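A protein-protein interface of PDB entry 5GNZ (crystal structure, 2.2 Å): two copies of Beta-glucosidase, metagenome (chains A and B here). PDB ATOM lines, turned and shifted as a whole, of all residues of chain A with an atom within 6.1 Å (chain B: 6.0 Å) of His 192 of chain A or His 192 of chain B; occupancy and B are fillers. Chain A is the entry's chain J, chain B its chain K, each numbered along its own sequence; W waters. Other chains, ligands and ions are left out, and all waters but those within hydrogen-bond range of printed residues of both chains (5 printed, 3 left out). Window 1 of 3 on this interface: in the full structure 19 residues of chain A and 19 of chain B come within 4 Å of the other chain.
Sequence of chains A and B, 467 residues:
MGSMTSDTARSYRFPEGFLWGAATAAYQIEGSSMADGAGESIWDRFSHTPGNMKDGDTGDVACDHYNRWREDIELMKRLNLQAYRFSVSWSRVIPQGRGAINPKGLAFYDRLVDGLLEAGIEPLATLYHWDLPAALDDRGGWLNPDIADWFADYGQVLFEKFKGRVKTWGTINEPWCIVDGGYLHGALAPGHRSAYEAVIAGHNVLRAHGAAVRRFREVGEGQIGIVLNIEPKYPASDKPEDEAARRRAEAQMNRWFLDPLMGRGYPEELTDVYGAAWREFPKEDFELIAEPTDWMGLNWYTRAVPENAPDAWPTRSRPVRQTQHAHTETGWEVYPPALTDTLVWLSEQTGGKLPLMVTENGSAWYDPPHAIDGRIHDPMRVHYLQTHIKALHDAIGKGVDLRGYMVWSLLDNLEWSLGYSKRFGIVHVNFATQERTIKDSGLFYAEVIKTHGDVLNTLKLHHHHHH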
ATOM      1  N   ASP A 137       1.076 -15.382  -4.075  1.00  0.00           N
ATOM      2  CA  ASP A 137       2.126 -15.286  -5.076  1.00  0.00           C
ATOM      3  C   ASP A 137       2.154 -16.543  -5.931  1.00  0.00           C
ATOM      4  O   ASP A 137       2.452 -16.487  -7.125  1.00  0.00           O
ATOM      5  CB  ASP A 137       3.486 -15.067  -4.415  1.00  0.00           C
ATOM      6  CG  ASP A 137       4.518 -14.508  -5.378  1.00  0.00           C
ATOM      7  OD1 ASP A 137       4.239 -13.461  -5.997  1.00  0.00           O
ATOM      8  OD2 ASP A 137       5.604 -15.110  -5.514  1.00  0.00           O
ATOM      9  N   GLY A 140      -0.033 -16.278  -8.770  1.00  0.00           N
ATOM     10  CA  GLY A 140       0.343 -15.274  -9.752  1.00  0.00           C
ATOM     11  C   GLY A 140       0.633 -13.908  -9.158  1.00  0.00           C
ATOM     12  O   GLY A 140       1.173 -13.030  -9.835  1.00  0.00           O
ATOM     13  N   LEU A 143       0.224 -10.271 -10.730  1.00  0.00           N
ATOM     14  CA  LEU A 143      -0.042 -10.535 -12.141  1.00  0.00           C
ATOM     15  C   LEU A 143      -1.450 -11.088 -12.328  1.00  0.00           C
ATOM     16  O   LEU A 143      -1.972 -11.113 -13.440  1.00  0.00           O
ATOM     17  CB  LEU A 143       0.988 -11.516 -12.704  1.00  0.00           C
ATOM     18  CG  LEU A 143       2.453 -11.098 -12.548  1.00  0.00           C
ATOM     19  CD1 LEU A 143       3.388 -12.164 -13.090  1.00  0.00           C
ATOM     20  CD2 LEU A 143       2.719  -9.759 -13.226  1.00  0.00           C
ATOM     21  N   VAL A 179       6.509  -2.570  -8.000  1.00  0.00           N
ATOM     22  CA  VAL A 179       6.523  -3.046  -9.383  1.00  0.00           C
ATOM     23  C   VAL A 179       7.909  -2.985 -10.038  1.00  0.00           C
ATOM     24  O   VAL A 179       8.365  -3.959 -10.637  1.00  0.00           O
ATOM     25  CB  VAL A 179       5.531  -2.232 -10.244  1.00  0.00           C
ATOM     26  CG1 VAL A 179       5.615  -2.653 -11.697  1.00  0.00           C
ATOM     27  CG2 VAL A 179       4.121  -2.392  -9.718  1.00  0.00           C
ATOM     28  N   ASP A 180       8.554  -1.828  -9.933  1.00  0.00           N
ATOM     29  CA  ASP A 180       9.884  -1.597 -10.487  1.00  0.00           C
ATOM     30  C   ASP A 180      10.935  -2.456  -9.794  1.00  0.00           C
ATOM     31  O   ASP A 180      11.796  -3.044 -10.451  1.00  0.00           O
ATOM     32  CB  ASP A 180      10.215  -0.089 -10.417  1.00  0.00           C
ATOM     33  CG  ASP A 180      11.557   0.263 -11.036  1.00  0.00           C
ATOM     34  OD1 ASP A 180      12.603  -0.042 -10.423  1.00  0.00           O
ATOM     35  OD2 ASP A 180      11.565   0.768 -12.179  1.00  0.00           O
ATOM     36  N   GLY A 181      10.846  -2.547  -8.474  1.00  0.00           N
ATOM     37  CA  GLY A 181      11.763  -3.373  -7.713  1.00  0.00           C
ATOM     38  C   GLY A 181      11.415  -4.850  -7.730  1.00  0.00           C
ATOM     39  O   GLY A 181      12.304  -5.702  -7.787  1.00  0.00           O
ATOM     40  N   GLY A 182      10.122  -5.163  -7.669  1.00  0.00           N
ATOM     41  CA  GLY A 182       9.691  -6.547  -7.563  1.00  0.00           C
ATOM     42  C   GLY A 182       9.469  -7.297  -8.862  1.00  0.00           C
ATOM     43  O   GLY A 182       9.604  -8.519  -8.909  1.00  0.00           O
ATOM     44  N   TYR A 183       9.115  -6.575  -9.920  1.00  0.00           N
ATOM     45  CA  TYR A 183       8.726  -7.225 -11.167  1.00  0.00           C
ATOM     46  C   TYR A 183       9.539  -6.769 -12.378  1.00  0.00           C
ATOM     47  O   TYR A 183       9.722  -7.530 -13.325  1.00  0.00           O
ATOM     48  CB  TYR A 183       7.231  -7.001 -11.424  1.00  0.00           C
ATOM     49  CG  TYR A 183       6.342  -7.821 -10.518  1.00  0.00           C
ATOM     50  CD1 TYR A 183       5.951  -7.342  -9.278  1.00  0.00           C
ATOM     51  CD2 TYR A 183       5.917  -9.083 -10.895  1.00  0.00           C
ATOM     52  CE1 TYR A 183       5.146  -8.088  -8.446  1.00  0.00           C
ATOM     53  CE2 TYR A 183       5.114  -9.842 -10.071  1.00  0.00           C
ATOM     54  CZ  TYR A 183       4.734  -9.338  -8.848  1.00  0.00           C
ATOM     55  OH  TYR A 183       3.932 -10.088  -8.023  1.00  0.00           O
ATOM     56  N   LEU A 184      10.022  -5.532 -12.353  1.00  0.00           N
ATOM     57  CA  LEU A 184      10.779  -5.007 -13.485  1.00  0.00           C
ATOM     58  C   LEU A 184      12.262  -5.371 -13.413  1.00  0.00           C
ATOM     59  O   LEU A 184      12.826  -5.883 -14.380  1.00  0.00           O
ATOM     60  CB  LEU A 184      10.611  -3.486 -13.577  1.00  0.00           C
ATOM     61  CG  LEU A 184      11.346  -2.794 -14.730  1.00  0.00           C
ATOM     62  CD1 LEU A 184      10.919  -3.367 -16.073  1.00  0.00           C
ATOM     63  CD2 LEU A 184      11.101  -1.288 -14.698  1.00  0.00           C
ATOM     64  N   HIS A 185      12.897  -5.106 -12.276  1.00  0.00           N
ATOM     65  CA  HIS A 185      14.335  -5.329 -12.154  1.00  0.00           C
ATOM     66  C   HIS A 185      14.714  -6.483 -11.215  1.00  0.00           C
ATOM     67  O   HIS A 185      15.832  -6.994 -11.285  1.00  0.00           O
ATOM     68  CB  HIS A 185      15.014  -4.030 -11.719  1.00  0.00           C
ATOM     69  CG  HIS A 185      14.925  -2.941 -12.746  1.00  0.00           C
ATOM     70  ND1 HIS A 185      15.585  -3.005 -13.954  1.00  0.00           N
ATOM     71  CD2 HIS A 185      14.231  -1.777 -12.758  1.00  0.00           C
ATOM     72  CE1 HIS A 185      15.313  -1.921 -14.662  1.00  0.00           C
ATOM     73  NE2 HIS A 185      14.495  -1.160 -13.958  1.00  0.00           N
ATOM     74  N   GLY A 186      13.794  -6.889 -10.343  1.00  0.00           N
ATOM     75  CA  GLY A 186      14.006  -8.059  -9.505  1.00  0.00           C
ATOM     76  C   GLY A 186      14.912  -7.913  -8.297  1.00  0.00           C
ATOM     77  O   GLY A 186      15.431  -8.907  -7.783  1.00  0.00           O
ATOM     78  N   ALA A 187      15.106  -6.685  -7.833  1.00  0.00           N
ATOM     79  CA  ALA A 187      15.932  -6.448  -6.656  1.00  0.00           C
ATOM     80  C   ALA A 187      15.127  -6.675  -5.379  1.00  0.00           C
ATOM     81  O   ALA A 187      15.690  -6.918  -4.318  1.00  0.00           O
ATOM     82  CB  ALA A 187      16.505  -5.036  -6.682  1.00  0.00           C
ATOM     83  N   LEU A 188      13.805  -6.604  -5.498  1.00  0.00           N
ATOM     84  CA  LEU A 188      12.897  -6.871  -4.385  1.00  0.00           C
ATOM     85  C   LEU A 188      12.030  -8.096  -4.665  1.00  0.00           C
ATOM     86  O   LEU A 188      11.873  -8.502  -5.816  1.00  0.00           O
ATOM     87  CB  LEU A 188      12.010  -5.649  -4.119  1.00  0.00           C
ATOM     88  CG  LEU A 188      12.739  -4.315  -3.940  1.00  0.00           C
ATOM     89  CD1 LEU A 188      11.755  -3.165  -3.803  1.00  0.00           C
ATOM     90  CD2 LEU A 188      13.672  -4.373  -2.742  1.00  0.00           C
ATOM     91  N   ALA A 189      11.484  -8.687  -3.604  1.00  0.00           N
ATOM     92  CA  ALA A 189      10.503  -9.764  -3.733  1.00  0.00           C
ATOM     93  C   ALA A 189       9.330  -9.326  -4.602  1.00  0.00           C
ATOM     94  O   ALA A 189       8.877  -8.188  -4.506  1.00  0.00           O
ATOM     95  CB  ALA A 189      10.007 -10.211  -2.359  1.00  0.00           C
ATOM     96  N   PRO A 190       8.822 -10.231  -5.456  1.00  0.00           N
ATOM     97  CA  PRO A 190       9.189 -11.647  -5.591  1.00  0.00           C
ATOM     98  C   PRO A 190      10.364 -11.900  -6.533  1.00  0.00           C
ATOM     99  O   PRO A 190      10.591 -13.045  -6.915  1.00  0.00           O
ATOM    100  CB  PRO A 190       7.911 -12.276  -6.155  1.00  0.00           C
ATOM    101  CG  PRO A 190       7.326 -11.187  -6.993  1.00  0.00           C
ATOM    102  CD  PRO A 190       7.674  -9.882  -6.313  1.00  0.00           C
ATOM    103  N   GLY A 191      11.093 -10.855  -6.904  1.00  0.00           N
ATOM    104  CA  GLY A 191      12.302 -11.028  -7.689  1.00  0.00           C
ATOM    105  C   GLY A 191      12.132 -11.396  -9.153  1.00  0.00           C
ATOM    106  O   GLY A 191      12.944 -12.138  -9.706  1.00  0.00           O
ATOM    107  N   HIS A 192      11.091 -10.878  -9.793  1.00  0.00           N
ATOM    108  CA  HIS A 192      10.932 -11.063 -11.233  1.00  0.00           C
ATOM    109  C   HIS A 192      11.602  -9.934 -12.004  1.00  0.00           C
ATOM    110  O   HIS A 192      11.732  -8.821 -11.499  1.00  0.00           O
ATOM    111  CB  HIS A 192       9.458 -11.132 -11.633  1.00  0.00           C
ATOM    112  CG  HIS A 192       8.700 -12.262 -11.008  1.00  0.00           C
ATOM    113  ND1 HIS A 192       7.474 -12.673 -11.485  1.00  0.00           N
ATOM    114  CD2 HIS A 192       8.989 -13.067  -9.960  1.00  0.00           C
ATOM    115  CE1 HIS A 192       7.039 -13.682 -10.753  1.00  0.00           C
ATOM    116  NE2 HIS A 192       7.935 -13.943  -9.822  1.00  0.00           N
ATOM    117  N   ARG A 193      12.009 -10.221 -13.236  1.00  0.00           N
ATOM    118  CA  ARG A 193      12.601  -9.205 -14.096  1.00  0.00           C
ATOM    119  C   ARG A 193      11.968  -9.271 -15.477  1.00  0.00           C
ATOM    120  O   ARG A 193      12.396 -10.043 -16.336  1.00  0.00           O
ATOM    121  CB  ARG A 193      14.118  -9.384 -14.183  1.00  0.00           C
ATOM    122  CG  ARG A 193      14.807  -8.362 -15.071  1.00  0.00           C
ATOM    123  CD  ARG A 193      16.315  -8.368 -14.865  1.00  0.00           C
ATOM    124  NE  ARG A 193      16.975  -7.397 -15.730  1.00  0.00           N
ATOM    125  CZ  ARG A 193      17.337  -7.652 -16.981  1.00  0.00           C
ATOM    126  NH1 ARG A 193      17.111  -8.848 -17.502  1.00  0.00           N
ATOM    127  NH2 ARG A 193      17.928  -6.718 -17.711  1.00  0.00           N
ATOM    128  N   SER A 194      10.943  -8.448 -15.677  1.00  0.00           N
ATOM    129  CA  SER A 194      10.130  -8.493 -16.886  1.00  0.00           C
ATOM    130  C   SER A 194       9.312  -7.217 -17.036  1.00  0.00           C
ATOM    131  O   SER A 194       8.572  -6.833 -16.129  1.00  0.00           O
ATOM    132  CB  SER A 194       9.206  -9.716 -16.858  1.00  0.00           C
ATOM    133  OG  SER A 194       8.363  -9.749 -17.993  1.00  0.00           O
ATOM    134  N   GLU A 197       5.536  -8.081 -17.197  1.00  0.00           N
ATOM    135  CA  GLU A 197       5.008  -8.329 -15.865  1.00  0.00           C
ATOM    136  C   GLU A 197       4.914  -7.016 -15.107  1.00  0.00           C
ATOM    137  O   GLU A 197       4.006  -6.829 -14.321  1.00  0.00           O
ATOM    138  CB  GLU A 197       5.880  -9.340 -15.108  1.00  0.00           C
ATOM    139  CG  GLU A 197       5.834 -10.758 -15.679  1.00  0.00           C
ATOM    140  CD  GLU A 197       6.619 -11.753 -14.846  1.00  0.00           C
ATOM    141  OE1 GLU A 197       6.872 -11.462 -13.661  1.00  0.00           O
ATOM    142  OE2 GLU A 197       6.985 -12.824 -15.377  1.00  0.00           O
ATOM    143  N   ASP B 137       0.946 -18.313 -16.570  1.00  0.00           N
ATOM    144  CA  ASP B 137       2.048 -17.844 -15.742  1.00  0.00           C
ATOM    145  C   ASP B 137       1.601 -16.665 -14.887  1.00  0.00           C
ATOM    146  O   ASP B 137       2.043 -16.507 -13.749  1.00  0.00           O
ATOM    147  CB  ASP B 137       3.251 -17.449 -16.598  1.00  0.00           C
ATOM    148  CG  ASP B 137       4.542 -17.405 -15.801  1.00  0.00           C
ATOM    149  OD1 ASP B 137       4.873 -18.423 -15.158  1.00  0.00           O
ATOM    150  OD2 ASP B 137       5.223 -16.357 -15.815  1.00  0.00           O
ATOM    151  N   GLY B 140       0.242 -17.889 -11.873  1.00  0.00           N
ATOM    152  CA  GLY B 140       1.176 -18.571 -10.995  1.00  0.00           C
ATOM    153  C   GLY B 140       1.932 -19.693 -11.676  1.00  0.00           C
ATOM    154  O   GLY B 140       2.913 -20.209 -11.138  1.00  0.00           O
ATOM    155  N   LEU B 143       3.413 -23.006 -10.159  1.00  0.00           N
ATOM    156  CA  LEU B 143       3.269 -22.810  -8.721  1.00  0.00           C
ATOM    157  C   LEU B 143       1.809 -22.933  -8.298  1.00  0.00           C
ATOM    158  O   LEU B 143       1.510 -23.095  -7.117  1.00  0.00           O
ATOM    159  CB  LEU B 143       3.813 -21.443  -8.308  1.00  0.00           C
ATOM    160  CG  LEU B 143       5.259 -21.115  -8.683  1.00  0.00           C
ATOM    161  CD1 LEU B 143       5.622 -19.706  -8.246  1.00  0.00           C
ATOM    162  CD2 LEU B 143       6.221 -22.123  -8.082  1.00  0.00           C
ATOM    163  N   VAL B 179      12.011 -27.122 -13.934  1.00  0.00           N
ATOM    164  CA  VAL B 179      11.998 -26.607 -12.570  1.00  0.00           C
ATOM    165  C   VAL B 179      13.335 -26.000 -12.138  1.00  0.00           C
ATOM    166  O   VAL B 179      13.387 -24.897 -11.600  1.00  0.00           O
ATOM    167  CB  VAL B 179      11.619 -27.719 -11.582  1.00  0.00           C
ATOM    168  CG1 VAL B 179      11.666 -27.197 -10.169  1.00  0.00           C
ATOM    169  CG2 VAL B 179      10.242 -28.255 -11.906  1.00  0.00           C
ATOM    170  N   ASP B 180      14.410 -26.743 -12.367  1.00  0.00           N
ATOM    171  CA  ASP B 180      15.756 -26.308 -12.022  1.00  0.00           C
ATOM    172  C   ASP B 180      16.174 -25.087 -12.835  1.00  0.00           C
ATOM    173  O   ASP B 180      16.792 -24.165 -12.304  1.00  0.00           O
ATOM    174  CB  ASP B 180      16.745 -27.470 -12.224  1.00  0.00           C
ATOM    175  CG  ASP B 180      18.162 -27.130 -11.793  1.00  0.00           C
ATOM    176  OD1 ASP B 180      18.796 -26.278 -12.447  1.00  0.00           O
ATOM    177  OD2 ASP B 180      18.655 -27.733 -10.818  1.00  0.00           O
ATOM    178  N   GLY B 181      15.864 -25.095 -14.126  1.00  0.00           N
ATOM    179  CA  GLY B 181      16.197 -23.972 -14.981  1.00  0.00           C
ATOM    180  C   GLY B 181      15.220 -22.819 -14.870  1.00  0.00           C
ATOM    181  O   GLY B 181      15.616 -21.650 -14.878  1.00  0.00           O
ATOM    182  N   GLY B 182      13.937 -23.149 -14.753  1.00  0.00           N
ATOM    183  CA  GLY B 182      12.900 -22.136 -14.770  1.00  0.00           C
ATOM    184  C   GLY B 182      12.559 -21.519 -13.428  1.00  0.00           C
ATOM    185  O   GLY B 182      12.095 -20.383 -13.368  1.00  0.00           O
ATOM    186  N   TYR B 183      12.768 -22.267 -12.350  1.00  0.00           N
ATOM    187  CA  TYR B 183      12.323 -21.819 -11.035  1.00  0.00           C
ATOM    188  C   TYR B 183      13.426 -21.778  -9.974  1.00  0.00           C
ATOM    189  O   TYR B 183      13.369 -20.971  -9.048  1.00  0.00           O
ATOM    190  CB  TYR B 183      11.167 -22.707 -10.565  1.00  0.00           C
ATOM    191  CG  TYR B 183       9.874 -22.427 -11.297  1.00  0.00           C
ATOM    192  CD1 TYR B 183       9.570 -23.070 -12.488  1.00  0.00           C
ATOM    193  CD2 TYR B 183       8.975 -21.496 -10.811  1.00  0.00           C
ATOM    194  CE1 TYR B 183       8.397 -22.811 -13.163  1.00  0.00           C
ATOM    195  CE2 TYR B 183       7.796 -21.224 -11.476  1.00  0.00           C
ATOM    196  CZ  TYR B 183       7.514 -21.884 -12.652  1.00  0.00           C
ATOM    197  OH  TYR B 183       6.345 -21.622 -13.322  1.00  0.00           O
ATOM    198  N   LEU B 184      14.427 -22.640 -10.102  1.00  0.00           N
ATOM    199  CA  LEU B 184      15.493 -22.695  -9.107  1.00  0.00           C
ATOM    200  C   LEU B 184      16.604 -21.681  -9.392  1.00  0.00           C
ATOM    201  O   LEU B 184      16.995 -20.916  -8.511  1.00  0.00           O
ATOM    202  CB  LEU B 184      16.083 -24.105  -9.034  1.00  0.00           C
ATOM    203  CG  LEU B 184      17.186 -24.300  -7.987  1.00  0.00           C
ATOM    204  CD1 LEU B 184      16.655 -23.976  -6.597  1.00  0.00           C
ATOM    205  CD2 LEU B 184      17.743 -25.715  -8.029  1.00  0.00           C
ATOM    206  N   HIS B 185      17.107 -21.674 -10.623  1.00  0.00           N
ATOM    207  CA  HIS B 185      18.248 -20.831 -10.970  1.00  0.00           C
ATOM    208  C   HIS B 185      17.899 -19.660 -11.894  1.00  0.00           C
ATOM    209  O   HIS B 185      18.651 -18.690 -11.974  1.00  0.00           O
ATOM    210  CB  HIS B 185      19.338 -21.695 -11.611  1.00  0.00           C
ATOM    211  CG  HIS B 185      19.922 -22.713 -10.682  1.00  0.00           C
ATOM    212  ND1 HIS B 185      20.691 -22.368  -9.593  1.00  0.00           N
ATOM    213  CD2 HIS B 185      19.842 -24.065 -10.676  1.00  0.00           C
ATOM    214  CE1 HIS B 185      21.064 -23.465  -8.957  1.00  0.00           C
ATOM    215  NE2 HIS B 185      20.564 -24.508  -9.594  1.00  0.00           N
ATOM    216  N   GLY B 186      16.770 -19.754 -12.588  1.00  0.00           N
ATOM    217  CA  GLY B 186      16.278 -18.653 -13.400  1.00  0.00           C
ATOM    218  C   GLY B 186      16.947 -18.427 -14.740  1.00  0.00           C
ATOM    219  O   GLY B 186      16.851 -17.339 -15.311  1.00  0.00           O
ATOM    220  N   ALA B 187      17.617 -19.448 -15.259  1.00  0.00           N
ATOM    221  CA  ALA B 187      18.271 -19.338 -16.558  1.00  0.00           C
ATOM    222  C   ALA B 187      17.276 -19.583 -17.688  1.00  0.00           C
ATOM    223  O   ALA B 187      17.494 -19.165 -18.822  1.00  0.00           O
ATOM    224  CB  ALA B 187      19.438 -20.317 -16.651  1.00  0.00           C
ATOM    225  N   LEU B 188      16.177 -20.254 -17.363  1.00  0.00           N
ATOM    226  CA  LEU B 188      15.107 -20.505 -18.320  1.00  0.00           C
ATOM    227  C   LEU B 188      13.822 -19.799 -17.908  1.00  0.00           C
ATOM    228  O   LEU B 188      13.646 -19.446 -16.743  1.00  0.00           O
ATOM    229  CB  LEU B 188      14.845 -22.010 -18.444  1.00  0.00           C
ATOM    230  CG  LEU B 188      16.027 -22.935 -18.733  1.00  0.00           C
ATOM    231  CD1 LEU B 188      15.585 -24.391 -18.686  1.00  0.00           C
ATOM    232  CD2 LEU B 188      16.664 -22.609 -20.075  1.00  0.00           C
ATOM    233  N   ALA B 189      12.931 -19.589 -18.872  1.00  0.00           N
ATOM    234  CA  ALA B 189      11.586 -19.094 -18.588  1.00  0.00           C
ATOM    235  C   ALA B 189      10.915 -20.010 -17.572  1.00  0.00           C
ATOM    236  O   ALA B 189      11.064 -21.230 -17.647  1.00  0.00           O
ATOM    237  CB  ALA B 189      10.760 -19.009 -19.867  1.00  0.00           C
ATOM    238  N   PRO B 190      10.161 -19.435 -16.618  1.00  0.00           N
ATOM    239  CA  PRO B 190       9.802 -18.017 -16.493  1.00  0.00           C
ATOM    240  C   PRO B 190      10.832 -17.172 -15.749  1.00  0.00           C
ATOM    241  O   PRO B 190      10.517 -16.048 -15.367  1.00  0.00           O
ATOM    242  CB  PRO B 190       8.488 -18.068 -15.709  1.00  0.00           C
ATOM    243  CG  PRO B 190       8.651 -19.260 -14.827  1.00  0.00           C
ATOM    244  CD  PRO B 190       9.481 -20.258 -15.600  1.00  0.00           C
ATOM    245  N   GLY B 191      12.032 -17.703 -15.542  1.00  0.00           N
ATOM    246  CA  GLY B 191      13.110 -16.927 -14.954  1.00  0.00           C
ATOM    247  C   GLY B 191      13.000 -16.642 -13.469  1.00  0.00           C
ATOM    248  O   GLY B 191      13.394 -15.570 -13.011  1.00  0.00           O
ATOM    249  N   HIS B 192      12.460 -17.587 -12.709  1.00  0.00           N
ATOM    250  CA  HIS B 192      12.442 -17.452 -11.255  1.00  0.00           C
ATOM    251  C   HIS B 192      13.678 -18.086 -10.628  1.00  0.00           C
ATOM    252  O   HIS B 192      14.233 -19.037 -11.170  1.00  0.00           O
ATOM    253  CB  HIS B 192      11.187 -18.096 -10.662  1.00  0.00           C
ATOM    254  CG  HIS B 192       9.901 -17.504 -11.156  1.00  0.00           C
ATOM    255  ND1 HIS B 192       8.696 -17.728 -10.526  1.00  0.00           N
ATOM    256  CD2 HIS B 192       9.636 -16.690 -12.204  1.00  0.00           C
ATOM    257  CE1 HIS B 192       7.740 -17.084 -11.173  1.00  0.00           C
ATOM    258  NE2 HIS B 192       8.281 -16.449 -12.194  1.00  0.00           N
ATOM    259  N   ARG B 193      14.087 -17.577  -9.469  1.00  0.00           N
ATOM    260  CA  ARG B 193      15.213 -18.151  -8.738  1.00  0.00           C
ATOM    261  C   ARG B 193      14.848 -18.310  -7.268  1.00  0.00           C
ATOM    262  O   ARG B 193      14.999 -17.383  -6.473  1.00  0.00           O
ATOM    263  CB  ARG B 193      16.467 -17.285  -8.892  1.00  0.00           C
ATOM    264  CG  ARG B 193      17.678 -17.816  -8.132  1.00  0.00           C
ATOM    265  CD  ARG B 193      18.967 -17.135  -8.560  1.00  0.00           C
ATOM    266  NE  ARG B 193      20.111 -17.640  -7.807  1.00  0.00           N
ATOM    267  CZ  ARG B 193      20.491 -17.172  -6.623  1.00  0.00           C
ATOM    268  NH1 ARG B 193      19.832 -16.167  -6.065  1.00  0.00           N
ATOM    269  NH2 ARG B 193      21.538 -17.694  -6.004  1.00  0.00           N
ATOM    270  N   SER B 194      14.363 -19.498  -6.921  1.00  0.00           N
ATOM    271  CA  SER B 194      13.829 -19.758  -5.589  1.00  0.00           C
ATOM    272  C   SER B 194      13.692 -21.253  -5.327  1.00  0.00           C
ATOM    273  O   SER B 194      13.052 -21.966  -6.101  1.00  0.00           O
ATOM    274  CB  SER B 194      12.474 -19.063  -5.422  1.00  0.00           C
ATOM    275  OG  SER B 194      11.907 -19.348  -4.156  1.00  0.00           O
ATOM    276  N   GLU B 197       9.999 -22.188  -4.483  1.00  0.00           N
ATOM    277  CA  GLU B 197       9.217 -22.264  -5.704  1.00  0.00           C
ATOM    278  C   GLU B 197       9.608 -23.501  -6.489  1.00  0.00           C
ATOM    279  O   GLU B 197       8.771 -24.109  -7.130  1.00  0.00           O
ATOM    280  CB  GLU B 197       9.404 -21.008  -6.561  1.00  0.00           C
ATOM    281  CG  GLU B 197       8.806 -19.737  -5.975  1.00  0.00           C
ATOM    282  CD  GLU B 197       8.927 -18.560  -6.921  1.00  0.00           C
ATOM    283  OE1 GLU B 197       9.108 -18.797  -8.133  1.00  0.00           O
ATOM    284  OE2 GLU B 197       8.847 -17.405  -6.453  1.00  0.00           O
HETATM  285  O   HOH W   1       7.704 -16.050  -4.181  1.00  0.00           O
HETATM  286  O   HOH W   2      12.010 -12.857 -13.838  1.00  0.00           O
HETATM  287  O   HOH W   3       9.568 -13.545 -15.303  1.00  0.00           O
HETATM  288  O   HOH W   4      12.817 -14.988  -8.447  1.00  0.00           O
HETATM  289  O   HOH W   5       6.563 -15.159 -13.851  1.00  0.00           O
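Among the printed residues, merely in contact across the chains: Gly 140 of chain A with Gly 140 of chain B and Glu 197 of chain A with Asp 137 of chain B.
Water W1 lies within hydrogen-bond range of the side-chain carboxylate (OD2) of Asp 137 of chain A (2.7 Å) and the side-chain carboxylate (OE2) of Glu 197 of chain B (2.9 Å). Water W5 lies within hydrogen-bond range of OD2 of Asp 137 of chain B, NE2 of His 192 of chain B and OE2 of Glu 197 of chain A. Water W3 lies within hydrogen-bond range of the backbone carbonyl oxygen (O) of Pro 190 of chain B and the side-chain carboxylate (OE2) of Glu 197 of chain A. Water W2 bridges N of Arg 193 of chain A (2.7 Å) and O of Gly 191 of chain B (3.2 Å). Water W4 lies within hydrogen-bond range of N of Arg 193 of chain B (3.1 Å), O of Gly 191 of chain A (3.1 Å) and O of Pro 190 of chain A (3.3 Å).
A ring nitrogen (NE2) of His 192 of chain A sits close to a ring nitrogen (NE2) of His 192 of chain B (3.5 Å).
Gly 140 of chain A touches its own counterpart, Gly 140 of chain B. His 192 of chain A touches its own counterpart, His 192 of chain B. Glu 197 of chain A touches Asp 137 of chain B, but with the chains exchanged Asp 137 of chain A does not touch Glu 197 of chain B (4.1 Å). 20 positions are printed for both chains. Of the 3 pairs that touch across the chains among the printed residues, 2 have their exchanged pair printed and touching as well.
Of the printed residues of chain B, Gly 140 of chain A touches Gly 140 (3.4 Å). Of chain B, only His 192 comes within 4 Å of His 192 of chain A. Ser 194 of chain A touches none of the printed residues of chain B. Printed residues of chain B within 4 Å of Glu 197 of chain A: Asp 137 (3.97 Å). Of the printed residues of chain A, Gly 140 of chain B touches Gly 140 (3.4 Å). Leu 143 of chain B touches none of the printed residues of chain A. Printed residues of chain A within 4 Å of His 192 of chain B: His 192. The nearest printed residue of chain B that does not touch Gly 140 of chain A is Asp 137 of chain B (4.5 Å).
Printed residues of chain A that touch a printed residue of chain B: Gly 140, His 192 and Glu 197. Hydrophobic or aromatic side chains of chain A within 4 Å of the printed part of chain B: His 192. Printed residues of chain B that touch a printed residue of chain A: Asp 137, Gly 140 and His 192. Hydrophobic or aromatic side chains of chain B within 4 Å of the printed part of chain A: His 192. Among the printed residues, 3 pairs touch across the chains.
The backbone NH (N) of Gly 186 of chain A lies within hydrogen-bond range of the backbone carbonyl oxygen (O) of His 192 of chain A (3.1 Å). O of Gly 182 of chain B sits at hydrogen-bond distance from N of His 192 of chain B (2.9 Å). O of Gly 182 of chain A is in hydrogen-bond range of N of His 192 of chain A (2.9 Å). ND1 of His 192 of chain B is in hydrogen-bond range of OE1 of Glu 197 of chain B (2.7 Å). OE1 of Glu 197 of chain A is in hydrogen-bond range of ND1 of His 192 of chain A (2.6 Å). OG of Ser 194 of chain A lies within hydrogen-bond range of N of Glu 197 of chain A.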
